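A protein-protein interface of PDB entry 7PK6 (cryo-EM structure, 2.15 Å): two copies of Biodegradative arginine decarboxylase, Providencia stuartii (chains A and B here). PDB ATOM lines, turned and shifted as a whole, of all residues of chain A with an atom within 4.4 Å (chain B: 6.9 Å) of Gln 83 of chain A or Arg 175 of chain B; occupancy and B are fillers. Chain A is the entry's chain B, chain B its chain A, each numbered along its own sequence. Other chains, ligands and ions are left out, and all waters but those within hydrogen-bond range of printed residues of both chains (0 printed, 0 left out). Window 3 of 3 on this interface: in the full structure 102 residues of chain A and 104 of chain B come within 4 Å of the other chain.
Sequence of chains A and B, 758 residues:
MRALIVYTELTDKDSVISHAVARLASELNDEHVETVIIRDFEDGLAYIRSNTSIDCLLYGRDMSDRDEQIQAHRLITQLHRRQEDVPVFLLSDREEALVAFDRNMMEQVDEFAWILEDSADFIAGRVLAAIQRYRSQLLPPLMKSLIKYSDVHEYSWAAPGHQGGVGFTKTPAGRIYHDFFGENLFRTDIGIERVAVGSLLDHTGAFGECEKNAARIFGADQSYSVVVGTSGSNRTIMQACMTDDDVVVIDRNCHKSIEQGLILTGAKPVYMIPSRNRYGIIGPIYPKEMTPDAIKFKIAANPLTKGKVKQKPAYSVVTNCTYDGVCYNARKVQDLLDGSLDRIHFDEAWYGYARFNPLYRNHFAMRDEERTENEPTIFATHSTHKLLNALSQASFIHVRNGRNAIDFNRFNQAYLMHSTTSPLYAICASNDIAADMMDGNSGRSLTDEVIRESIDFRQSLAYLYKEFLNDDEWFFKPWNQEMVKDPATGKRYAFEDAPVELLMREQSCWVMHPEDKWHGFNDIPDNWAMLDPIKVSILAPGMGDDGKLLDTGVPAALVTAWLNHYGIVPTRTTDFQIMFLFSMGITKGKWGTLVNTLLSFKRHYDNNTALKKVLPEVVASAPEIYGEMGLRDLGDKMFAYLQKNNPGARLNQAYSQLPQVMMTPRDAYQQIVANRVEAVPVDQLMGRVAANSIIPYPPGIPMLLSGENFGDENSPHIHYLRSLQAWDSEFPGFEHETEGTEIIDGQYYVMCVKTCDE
The backbone carbonyl oxygen (O) of Lys 170 of chain B lies close to the side-chain amide oxygen (OD1) of Asn 51 of chain A (3.3 Å). The side-chain hydroxyl (OG) of Ser 53 of chain A lies within hydrogen-bond range of the guanidinium group (NH2) of Arg 175 of chain B, 3.4 Å away.
N of Arg 175 of chain B lies within hydrogen-bond range of O of Phe 168 of chain B, at 3.5 Å. N of Ile 54 of chain A sits at hydrogen-bond distance from OE1 of Gln 83 of chain A (2.7 Å).
Among the printed residues, pairs that only touch across the chains: Ser 53 of chain A with Pro 172 of chain B (3.4 Å), Arg 82 of chain A with Pro 172 of chain B (3.4 Å), Arg 82 of chain A with Lys 170 of chain B (3.5 Å), Asn 51 of chain A with Thr 169 of chain B (3.5 Å), Asn 51 of chain A with Arg 175 of chain B (3.5 Å), Gln 83 of chain A with Pro 172 of chain B (3.6 Å), Thr 52 of chain A with Arg 175 of chain B (3.8 Å) and Gln 83 of chain A with Arg 175 of chain B (3.9 Å).
Gln 83 of chain A touches just these residues of chain B: Pro 172 and Arg 175. Arg 175 of chain B touches just these residues of chain A: Asn 51 (3.5 Å), Thr 52 (3.8 Å), Ser 53 (3.4 Å) and Gln 83 (3.9 Å). Of the printed residues of chain B, Thr 52 of chain A touches Arg 175 (3.8 Å). Printed residues of chain B within 4 Å of Ser 53 of chain A: Pro 172 and Arg 175. Thr 171 of chain B touches none of the printed residues of chain A. The nearest residue of chain B that does not touch Gln 83 of chain A is Thr 171 of chain B (5.7 Å). The nearest printed residue of chain A that does not touch Arg 175 of chain B is Ile 54 of chain A (5.1 Å). The nearest printed residue of chain A that does not touch Thr 169 of chain B is Thr 52 of chain A (6.4 Å).
Among the printed residues, no Asp or Glu carboxylate lies within 4 Å of a Lys or Arg side-chain nitrogen of the other chain.
No position is printed for both chains.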
ATOM      1  N   ASN A  51     -16.602 -12.302 -27.900  1.00  0.00           N
ATOM      2  CA  ASN A  51     -17.120 -12.858 -26.650  1.00  0.00           C
ATOM      3  C   ASN A  51     -17.809 -11.756 -25.842  1.00  0.00           C
ATOM      4  O   ASN A  51     -17.382 -11.360 -24.756  1.00  0.00           O
ATOM      5  CB  ASN A  51     -15.999 -13.525 -25.864  1.00  0.00           C
ATOM      6  CG  ASN A  51     -15.627 -14.885 -26.423  1.00  0.00           C
ATOM      7  OD1 ASN A  51     -16.468 -15.778 -26.527  1.00  0.00           O
ATOM      8  ND2 ASN A  51     -14.366 -15.042 -26.803  1.00  0.00           N
ATOM      9  N   THR A  52     -18.911 -11.265 -26.399  1.00  0.00           N
ATOM     10  CA  THR A  52     -19.743 -10.250 -25.768  1.00  0.00           C
ATOM     11  C   THR A  52     -21.059 -10.884 -25.349  1.00  0.00           C
ATOM     12  O   THR A  52     -21.682 -11.604 -26.136  1.00  0.00           O
ATOM     13  CB  THR A  52     -19.999  -9.077 -26.716  1.00  0.00           C
ATOM     14  OG1 THR A  52     -18.754  -8.472 -27.079  1.00  0.00           O
ATOM     15  CG2 THR A  52     -20.882  -8.037 -26.054  1.00  0.00           C
ATOM     16  N   SER A  53     -21.476 -10.625 -24.116  1.00  0.00           N
ATOM     17  CA  SER A  53     -22.718 -11.197 -23.620  1.00  0.00           C
ATOM     18  C   SER A  53     -23.912 -10.549 -24.304  1.00  0.00           C
ATOM     19  O   SER A  53     -24.036  -9.322 -24.335  1.00  0.00           O
ATOM     20  CB  SER A  53     -22.817 -11.020 -22.107  1.00  0.00           C
ATOM     21  OG  SER A  53     -22.925 -12.273 -21.462  1.00  0.00           O
ATOM     22  N   ILE A  54     -24.789 -11.376 -24.859  1.00  0.00           N
ATOM     23  CA  ILE A  54     -26.003 -10.921 -25.520  1.00  0.00           C
ATOM     24  C   ILE A  54     -27.177 -11.533 -24.776  1.00  0.00           C
ATOM     25  O   ILE A  54     -27.242 -12.757 -24.615  1.00  0.00           O
ATOM     26  CB  ILE A  54     -26.024 -11.301 -27.008  1.00  0.00           C
ATOM     27  CG1 ILE A  54     -24.964 -10.505 -27.770  1.00  0.00           C
ATOM     28  CG2 ILE A  54     -27.398 -11.064 -27.605  1.00  0.00           C
ATOM     29  CD1 ILE A  54     -24.382 -11.231 -28.950  1.00  0.00           C
ATOM     30  N   LEU A  79     -25.077 -17.924 -32.481  1.00  0.00           N
ATOM     31  CA  LEU A  79     -25.355 -17.342 -31.173  1.00  0.00           C
ATOM     32  C   LEU A  79     -25.551 -18.423 -30.122  1.00  0.00           C
ATOM     33  O   LEU A  79     -25.027 -18.321 -29.008  1.00  0.00           O
ATOM     34  CB  LEU A  79     -26.586 -16.443 -31.241  1.00  0.00           C
ATOM     35  CG  LEU A  79     -27.211 -16.063 -29.897  1.00  0.00           C
ATOM     36  CD1 LEU A  79     -26.370 -15.011 -29.199  1.00  0.00           C
ATOM     37  CD2 LEU A  79     -28.636 -15.583 -30.073  1.00  0.00           C
ATOM     38  N   HIS A  80     -26.281 -19.477 -30.460  1.00  0.00           N
ATOM     39  CA  HIS A  80     -26.552 -20.514 -29.477  1.00  0.00           C
ATOM     40  C   HIS A  80     -25.401 -21.494 -29.299  1.00  0.00           C
ATOM     41  O   HIS A  80     -25.494 -22.365 -28.431  1.00  0.00           O
ATOM     42  CB  HIS A  80     -27.833 -21.256 -29.846  1.00  0.00           C
ATOM     43  CG  HIS A  80     -29.069 -20.450 -29.614  1.00  0.00           C
ATOM     44  ND1 HIS A  80     -30.266 -20.719 -30.237  1.00  0.00           N
ATOM     45  CD2 HIS A  80     -29.289 -19.366 -28.833  1.00  0.00           C
ATOM     46  CE1 HIS A  80     -31.172 -19.844 -29.843  1.00  0.00           C
ATOM     47  NE2 HIS A  80     -30.604 -19.012 -28.991  1.00  0.00           N
ATOM     48  N   ARG A  81     -24.337 -21.390 -30.097  1.00  0.00           N
ATOM     49  CA  ARG A  81     -23.150 -22.203 -29.841  1.00  0.00           C
ATOM     50  C   ARG A  81     -22.612 -21.980 -28.429  1.00  0.00           C
ATOM     51  O   ARG A  81     -22.370 -22.937 -27.688  1.00  0.00           O
ATOM     52  CB  ARG A  81     -22.060 -21.904 -30.872  1.00  0.00           C
ATOM     53  CG  ARG A  81     -22.359 -22.397 -32.269  1.00  0.00           C
ATOM     54  CD  ARG A  81     -21.609 -23.669 -32.575  1.00  0.00           C
ATOM     55  NE  ARG A  81     -20.193 -23.427 -32.832  1.00  0.00           N
ATOM     56  CZ  ARG A  81     -19.271 -24.381 -32.864  1.00  0.00           C
ATOM     57  NH1 ARG A  81     -19.611 -25.644 -32.653  1.00  0.00           N
ATOM     58  NH2 ARG A  81     -18.007 -24.074 -33.103  1.00  0.00           N
ATOM     59  N   ARG A  82     -22.419 -20.723 -28.036  1.00  0.00           N
ATOM     60  CA  ARG A  82     -21.897 -20.404 -26.717  1.00  0.00           C
ATOM     61  C   ARG A  82     -22.879 -19.674 -25.817  1.00  0.00           C
ATOM     62  O   ARG A  82     -22.608 -19.545 -24.621  1.00  0.00           O
ATOM     63  CB  ARG A  82     -20.618 -19.562 -26.831  1.00  0.00           C
ATOM     64  CG  ARG A  82     -19.357 -20.382 -26.744  1.00  0.00           C
ATOM     65  CD  ARG A  82     -18.196 -19.652 -27.347  1.00  0.00           C
ATOM     66  NE  ARG A  82     -17.236 -20.575 -27.933  1.00  0.00           N
ATOM     67  CZ  ARG A  82     -15.956 -20.290 -28.125  1.00  0.00           C
ATOM     68  NH1 ARG A  82     -15.485 -19.105 -27.767  1.00  0.00           N
ATOM     69  NH2 ARG A  82     -15.150 -21.187 -28.667  1.00  0.00           N
ATOM     70  N   GLN A  83     -23.999 -19.190 -26.345  1.00  0.00           N
ATOM     71  CA  GLN A  83     -25.033 -18.529 -25.554  1.00  0.00           C
ATOM     72  C   GLN A  83     -26.337 -19.247 -25.886  1.00  0.00           C
ATOM     73  O   GLN A  83     -27.129 -18.787 -26.707  1.00  0.00           O
ATOM     74  CB  GLN A  83     -25.072 -17.043 -25.862  1.00  0.00           C
ATOM     75  CG  GLN A  83     -23.789 -16.336 -25.463  1.00  0.00           C
ATOM     76  CD  GLN A  83     -23.698 -14.914 -25.962  1.00  0.00           C
ATOM     77  OE1 GLN A  83     -24.181 -13.991 -25.317  1.00  0.00           O
ATOM     78  NE2 GLN A  83     -23.046 -14.726 -27.096  1.00  0.00           N
ATOM     79  N   GLU A  84     -26.571 -20.361 -25.195  1.00  0.00           N
ATOM     80  CA  GLU A  84     -27.451 -21.403 -25.714  1.00  0.00           C
ATOM     81  C   GLU A  84     -28.923 -21.009 -25.669  1.00  0.00           C
ATOM     82  O   GLU A  84     -29.668 -21.284 -26.616  1.00  0.00           O
ATOM     83  CB  GLU A  84     -27.224 -22.698 -24.941  1.00  0.00           C
ATOM     84  CG  GLU A  84     -27.778 -23.928 -25.618  1.00  0.00           C
ATOM     85  CD  GLU A  84     -27.456 -25.198 -24.860  1.00  0.00           C
ATOM     86  OE1 GLU A  84     -28.203 -25.536 -23.920  1.00  0.00           O
ATOM     87  OE2 GLU A  84     -26.451 -25.856 -25.194  1.00  0.00           O
ATOM     88  N   ASP A  85     -29.380 -20.402 -24.581  1.00  0.00           N
ATOM     89  CA  ASP A  85     -30.809 -20.179 -24.389  1.00  0.00           C
ATOM     90  C   ASP A  85     -31.198 -18.710 -24.512  1.00  0.00           C
ATOM     91  O   ASP A  85     -32.205 -18.285 -23.945  1.00  0.00           O
ATOM     92  CB  ASP A  85     -31.255 -20.737 -23.040  1.00  0.00           C
ATOM     93  CG  ASP A  85     -31.055 -22.232 -22.936  1.00  0.00           C
ATOM     94  OD1 ASP A  85     -31.781 -22.978 -23.628  1.00  0.00           O
ATOM     95  OD2 ASP A  85     -30.174 -22.667 -22.164  1.00  0.00           O
ATOM     96  N   VAL A  86     -30.418 -17.928 -25.244  1.00  0.00           N
ATOM     97  CA  VAL A  86     -30.746 -16.511 -25.434  1.00  0.00           C
ATOM     98  C   VAL A  86     -32.061 -16.399 -26.199  1.00  0.00           C
ATOM     99  O   VAL A  86     -32.228 -17.065 -27.235  1.00  0.00           O
ATOM    100  CB  VAL A  86     -29.612 -15.798 -26.170  1.00  0.00           C
ATOM    101  CG1 VAL A  86     -30.043 -14.408 -26.605  1.00  0.00           C
ATOM    102  CG2 VAL A  86     -28.390 -15.716 -25.286  1.00  0.00           C
ATOM    103  N   PHE B 168     -12.472 -18.203 -18.709  1.00  0.00           N
ATOM    104  CA  PHE B 168     -13.819 -18.015 -18.180  1.00  0.00           C
ATOM    105  C   PHE B 168     -14.633 -17.041 -19.020  1.00  0.00           C
ATOM    106  O   PHE B 168     -15.853 -17.186 -19.119  1.00  0.00           O
ATOM    107  CB  PHE B 168     -13.759 -17.531 -16.732  1.00  0.00           C
ATOM    108  CG  PHE B 168     -13.134 -18.512 -15.794  1.00  0.00           C
ATOM    109  CD1 PHE B 168     -13.793 -19.674 -15.447  1.00  0.00           C
ATOM    110  CD2 PHE B 168     -11.885 -18.272 -15.255  1.00  0.00           C
ATOM    111  CE1 PHE B 168     -13.216 -20.574 -14.586  1.00  0.00           C
ATOM    112  CE2 PHE B 168     -11.307 -19.170 -14.394  1.00  0.00           C
ATOM    113  CZ  PHE B 168     -11.970 -20.322 -14.059  1.00  0.00           C
ATOM    114  N   THR B 169     -13.989 -16.056 -19.642  1.00  0.00           N
ATOM    115  CA  THR B 169     -14.732 -15.026 -20.354  1.00  0.00           C
ATOM    116  C   THR B 169     -15.088 -15.451 -21.772  1.00  0.00           C
ATOM    117  O   THR B 169     -14.890 -14.686 -22.717  1.00  0.00           O
ATOM    118  CB  THR B 169     -13.923 -13.731 -20.405  1.00  0.00           C
ATOM    119  OG1 THR B 169     -12.940 -13.830 -21.441  1.00  0.00           O
ATOM    120  CG2 THR B 169     -13.224 -13.481 -19.079  1.00  0.00           C
ATOM    121  N   LYS B 170     -15.645 -16.645 -21.930  1.00  0.00           N
ATOM    122  CA  LYS B 170     -16.066 -17.131 -23.235  1.00  0.00           C
ATOM    123  C   LYS B 170     -17.503 -17.613 -23.272  1.00  0.00           C
ATOM    124  O   LYS B 170     -18.044 -17.781 -24.368  1.00  0.00           O
ATOM    125  CB  LYS B 170     -15.139 -18.256 -23.716  1.00  0.00           C
ATOM    126  CG  LYS B 170     -13.831 -17.736 -24.274  1.00  0.00           C
ATOM    127  CD  LYS B 170     -12.861 -18.842 -24.602  1.00  0.00           C
ATOM    128  CE  LYS B 170     -11.590 -18.271 -25.203  1.00  0.00           C
ATOM    129  NZ  LYS B 170     -10.723 -19.319 -25.792  1.00  0.00           N
ATOM    130  N   THR B 171     -18.132 -17.836 -22.129  1.00  0.00           N
ATOM    131  CA  THR B 171     -19.563 -18.044 -22.005  1.00  0.00           C
ATOM    132  C   THR B 171     -20.132 -16.957 -21.104  1.00  0.00           C
ATOM    133  O   THR B 171     -19.398 -16.346 -20.320  1.00  0.00           O
ATOM    134  CB  THR B 171     -19.886 -19.427 -21.423  1.00  0.00           C
ATOM    135  OG1 THR B 171     -19.348 -19.532 -20.102  1.00  0.00           O
ATOM    136  CG2 THR B 171     -19.297 -20.522 -22.292  1.00  0.00           C
ATOM    137  N   PRO B 172     -21.427 -16.655 -21.221  1.00  0.00           N
ATOM    138  CA  PRO B 172     -22.008 -15.634 -20.332  1.00  0.00           C
ATOM    139  C   PRO B 172     -21.914 -15.980 -18.854  1.00  0.00           C
ATOM    140  O   PRO B 172     -21.612 -15.100 -18.038  1.00  0.00           O
ATOM    141  CB  PRO B 172     -23.466 -15.539 -20.809  1.00  0.00           C
ATOM    142  CG  PRO B 172     -23.674 -16.684 -21.733  1.00  0.00           C
ATOM    143  CD  PRO B 172     -22.356 -17.057 -22.287  1.00  0.00           C
ATOM    144  N   ALA B 173     -22.154 -17.240 -18.483  1.00  0.00           N
ATOM    145  CA  ALA B 173     -22.031 -17.626 -17.081  1.00  0.00           C
ATOM    146  C   ALA B 173     -20.591 -17.504 -16.605  1.00  0.00           C
ATOM    147  O   ALA B 173     -20.337 -17.041 -15.488  1.00  0.00           O
ATOM    148  CB  ALA B 173     -22.547 -19.046 -16.874  1.00  0.00           C
ATOM    149  N   GLY B 174     -19.640 -17.914 -17.442  1.00  0.00           N
ATOM    150  CA  GLY B 174     -18.244 -17.706 -17.123  1.00  0.00           C
ATOM    151  C   GLY B 174     -17.888 -16.245 -16.955  1.00  0.00           C
ATOM    152  O   GLY B 174     -17.080 -15.902 -16.095  1.00  0.00           O
ATOM    153  N   ARG B 175     -18.482 -15.366 -17.765  1.00  0.00           N
ATOM    154  CA  ARG B 175     -18.210 -13.940 -17.629  1.00  0.00           C
ATOM    155  C   ARG B 175     -18.772 -13.390 -16.325  1.00  0.00           C
ATOM    156  O   ARG B 175     -18.126 -12.572 -15.663  1.00  0.00           O
ATOM    157  CB  ARG B 175     -18.774 -13.174 -18.829  1.00  0.00           C
ATOM    158  CG  ARG B 175     -17.913 -13.281 -20.077  1.00  0.00           C
ATOM    159  CD  ARG B 175     -18.357 -12.332 -21.186  1.00  0.00           C
ATOM    160  NE  ARG B 175     -19.569 -12.782 -21.865  1.00  0.00           N
ATOM    161  CZ  ARG B 175     -19.603 -13.723 -22.802  1.00  0.00           C
ATOM    162  NH1 ARG B 175     -18.489 -14.329 -23.183  1.00  0.00           N
ATOM    163  NH2 ARG B 175     -20.755 -14.059 -23.361  1.00  0.00           N
ATOM    164  N   ILE B 176     -19.967 -13.836 -15.935  1.00  0.00           N
ATOM    165  CA  ILE B 176     -20.526 -13.423 -14.649  1.00  0.00           C
ATOM    166  C   ILE B 176     -19.635 -13.895 -13.505  1.00  0.00           C
ATOM    167  O   ILE B 176     -19.330 -13.134 -12.579  1.00  0.00           O
ATOM    168  CB  ILE B 176     -21.965 -13.948 -14.505  1.00  0.00           C
ATOM    169  CG1 ILE B 176     -22.906 -13.155 -15.412  1.00  0.00           C
ATOM    170  CG2 ILE B 176     -22.424 -13.891 -13.057  1.00  0.00           C
ATOM    171  CD1 ILE B 176     -24.289 -13.729 -15.490  1.00  0.00           C
ATOM    172  N   TYR B 177     -19.191 -15.150 -13.563  1.00  0.00           N
ATOM    173  CA  TYR B 177     -18.310 -15.695 -12.536  1.00  0.00           C
ATOM    174  C   TYR B 177     -16.994 -14.926 -12.465  1.00  0.00           C
ATOM    175  O   TYR B 177     -16.511 -14.590 -11.374  1.00  0.00           O
ATOM    176  CB  TYR B 177     -18.080 -17.179 -12.832  1.00  0.00           C
ATOM    177  CG  TYR B 177     -16.903 -17.820 -12.146  1.00  0.00           C
ATOM    178  CD1 TYR B 177     -17.047 -18.442 -10.917  1.00  0.00           C
ATOM    179  CD2 TYR B 177     -15.653 -17.834 -12.745  1.00  0.00           C
ATOM    180  CE1 TYR B 177     -15.977 -19.039 -10.295  1.00  0.00           C
ATOM    181  CE2 TYR B 177     -14.581 -18.422 -12.132  1.00  0.00           C
ATOM    182  CZ  TYR B 177     -14.746 -19.023 -10.908  1.00  0.00           C
ATOM    183  OH  TYR B 177     -13.671 -19.609 -10.299  1.00  0.00           O
ATOM    184  N   HIS B 178     -16.412 -14.625 -13.626  1.00  0.00           N
ATOM    185  CA  HIS B 178     -15.147 -13.908 -13.692  1.00  0.00           C
ATOM    186  C   HIS B 178     -15.278 -12.497 -13.141  1.00  0.00           C
ATOM    187  O   HIS B 178     -14.387 -12.018 -12.434  1.00  0.00           O
ATOM    188  CB  HIS B 178     -14.660 -13.883 -15.140  1.00  0.00           C
ATOM    189  CG  HIS B 178     -13.375 -13.148 -15.340  1.00  0.00           C
ATOM    190  ND1 HIS B 178     -13.326 -11.798 -15.607  1.00  0.00           N
ATOM    191  CD2 HIS B 178     -12.092 -13.575 -15.327  1.00  0.00           C
ATOM    192  CE1 HIS B 178     -12.067 -11.424 -15.741  1.00  0.00           C
ATOM    193  NE2 HIS B 178     -11.298 -12.484 -15.578  1.00  0.00           N
ATOM    194  N   ASP B 179     -16.374 -11.810 -13.460  1.00  0.00           N
ATOM    195  CA  ASP B 179     -16.581 -10.472 -12.923  1.00  0.00           C
ATOM    196  C   ASP B 179     -16.838 -10.505 -11.424  1.00  0.00           C
ATOM    197  O   ASP B 179     -16.409  -9.598 -10.707  1.00  0.00           O
ATOM    198  CB  ASP B 179     -17.734  -9.784 -13.649  1.00  0.00           C
ATOM    199  CG  ASP B 179     -17.376  -9.399 -15.069  1.00  0.00           C
ATOM    200  OD1 ASP B 179     -16.176  -9.182 -15.341  1.00  0.00           O
ATOM    201  OD2 ASP B 179     -18.291  -9.317 -15.916  1.00  0.00           O
ATOM    202  N   PHE B 180     -17.533 -11.532 -10.936  1.00  0.00           N
ATOM    203  CA  PHE B 180     -17.777 -11.641  -9.504  1.00  0.00           C
ATOM    204  C   PHE B 180     -16.475 -11.823  -8.736  1.00  0.00           C
ATOM    205  O   PHE B 180     -16.211 -11.101  -7.770  1.00  0.00           O
ATOM    206  CB  PHE B 180     -18.734 -12.795  -9.220  1.00  0.00           C
ATOM    207  CG  PHE B 180     -19.057 -12.967  -7.765  1.00  0.00           C
ATOM    208  CD1 PHE B 180     -19.951 -12.119  -7.136  1.00  0.00           C
ATOM    209  CD2 PHE B 180     -18.463 -13.972  -7.025  1.00  0.00           C
ATOM    210  CE1 PHE B 180     -20.248 -12.275  -5.800  1.00  0.00           C
ATOM    211  CE2 PHE B 180     -18.755 -14.130  -5.688  1.00  0.00           C
ATOM    212  CZ  PHE B 180     -19.649 -13.281  -5.074  1.00  0.00           C
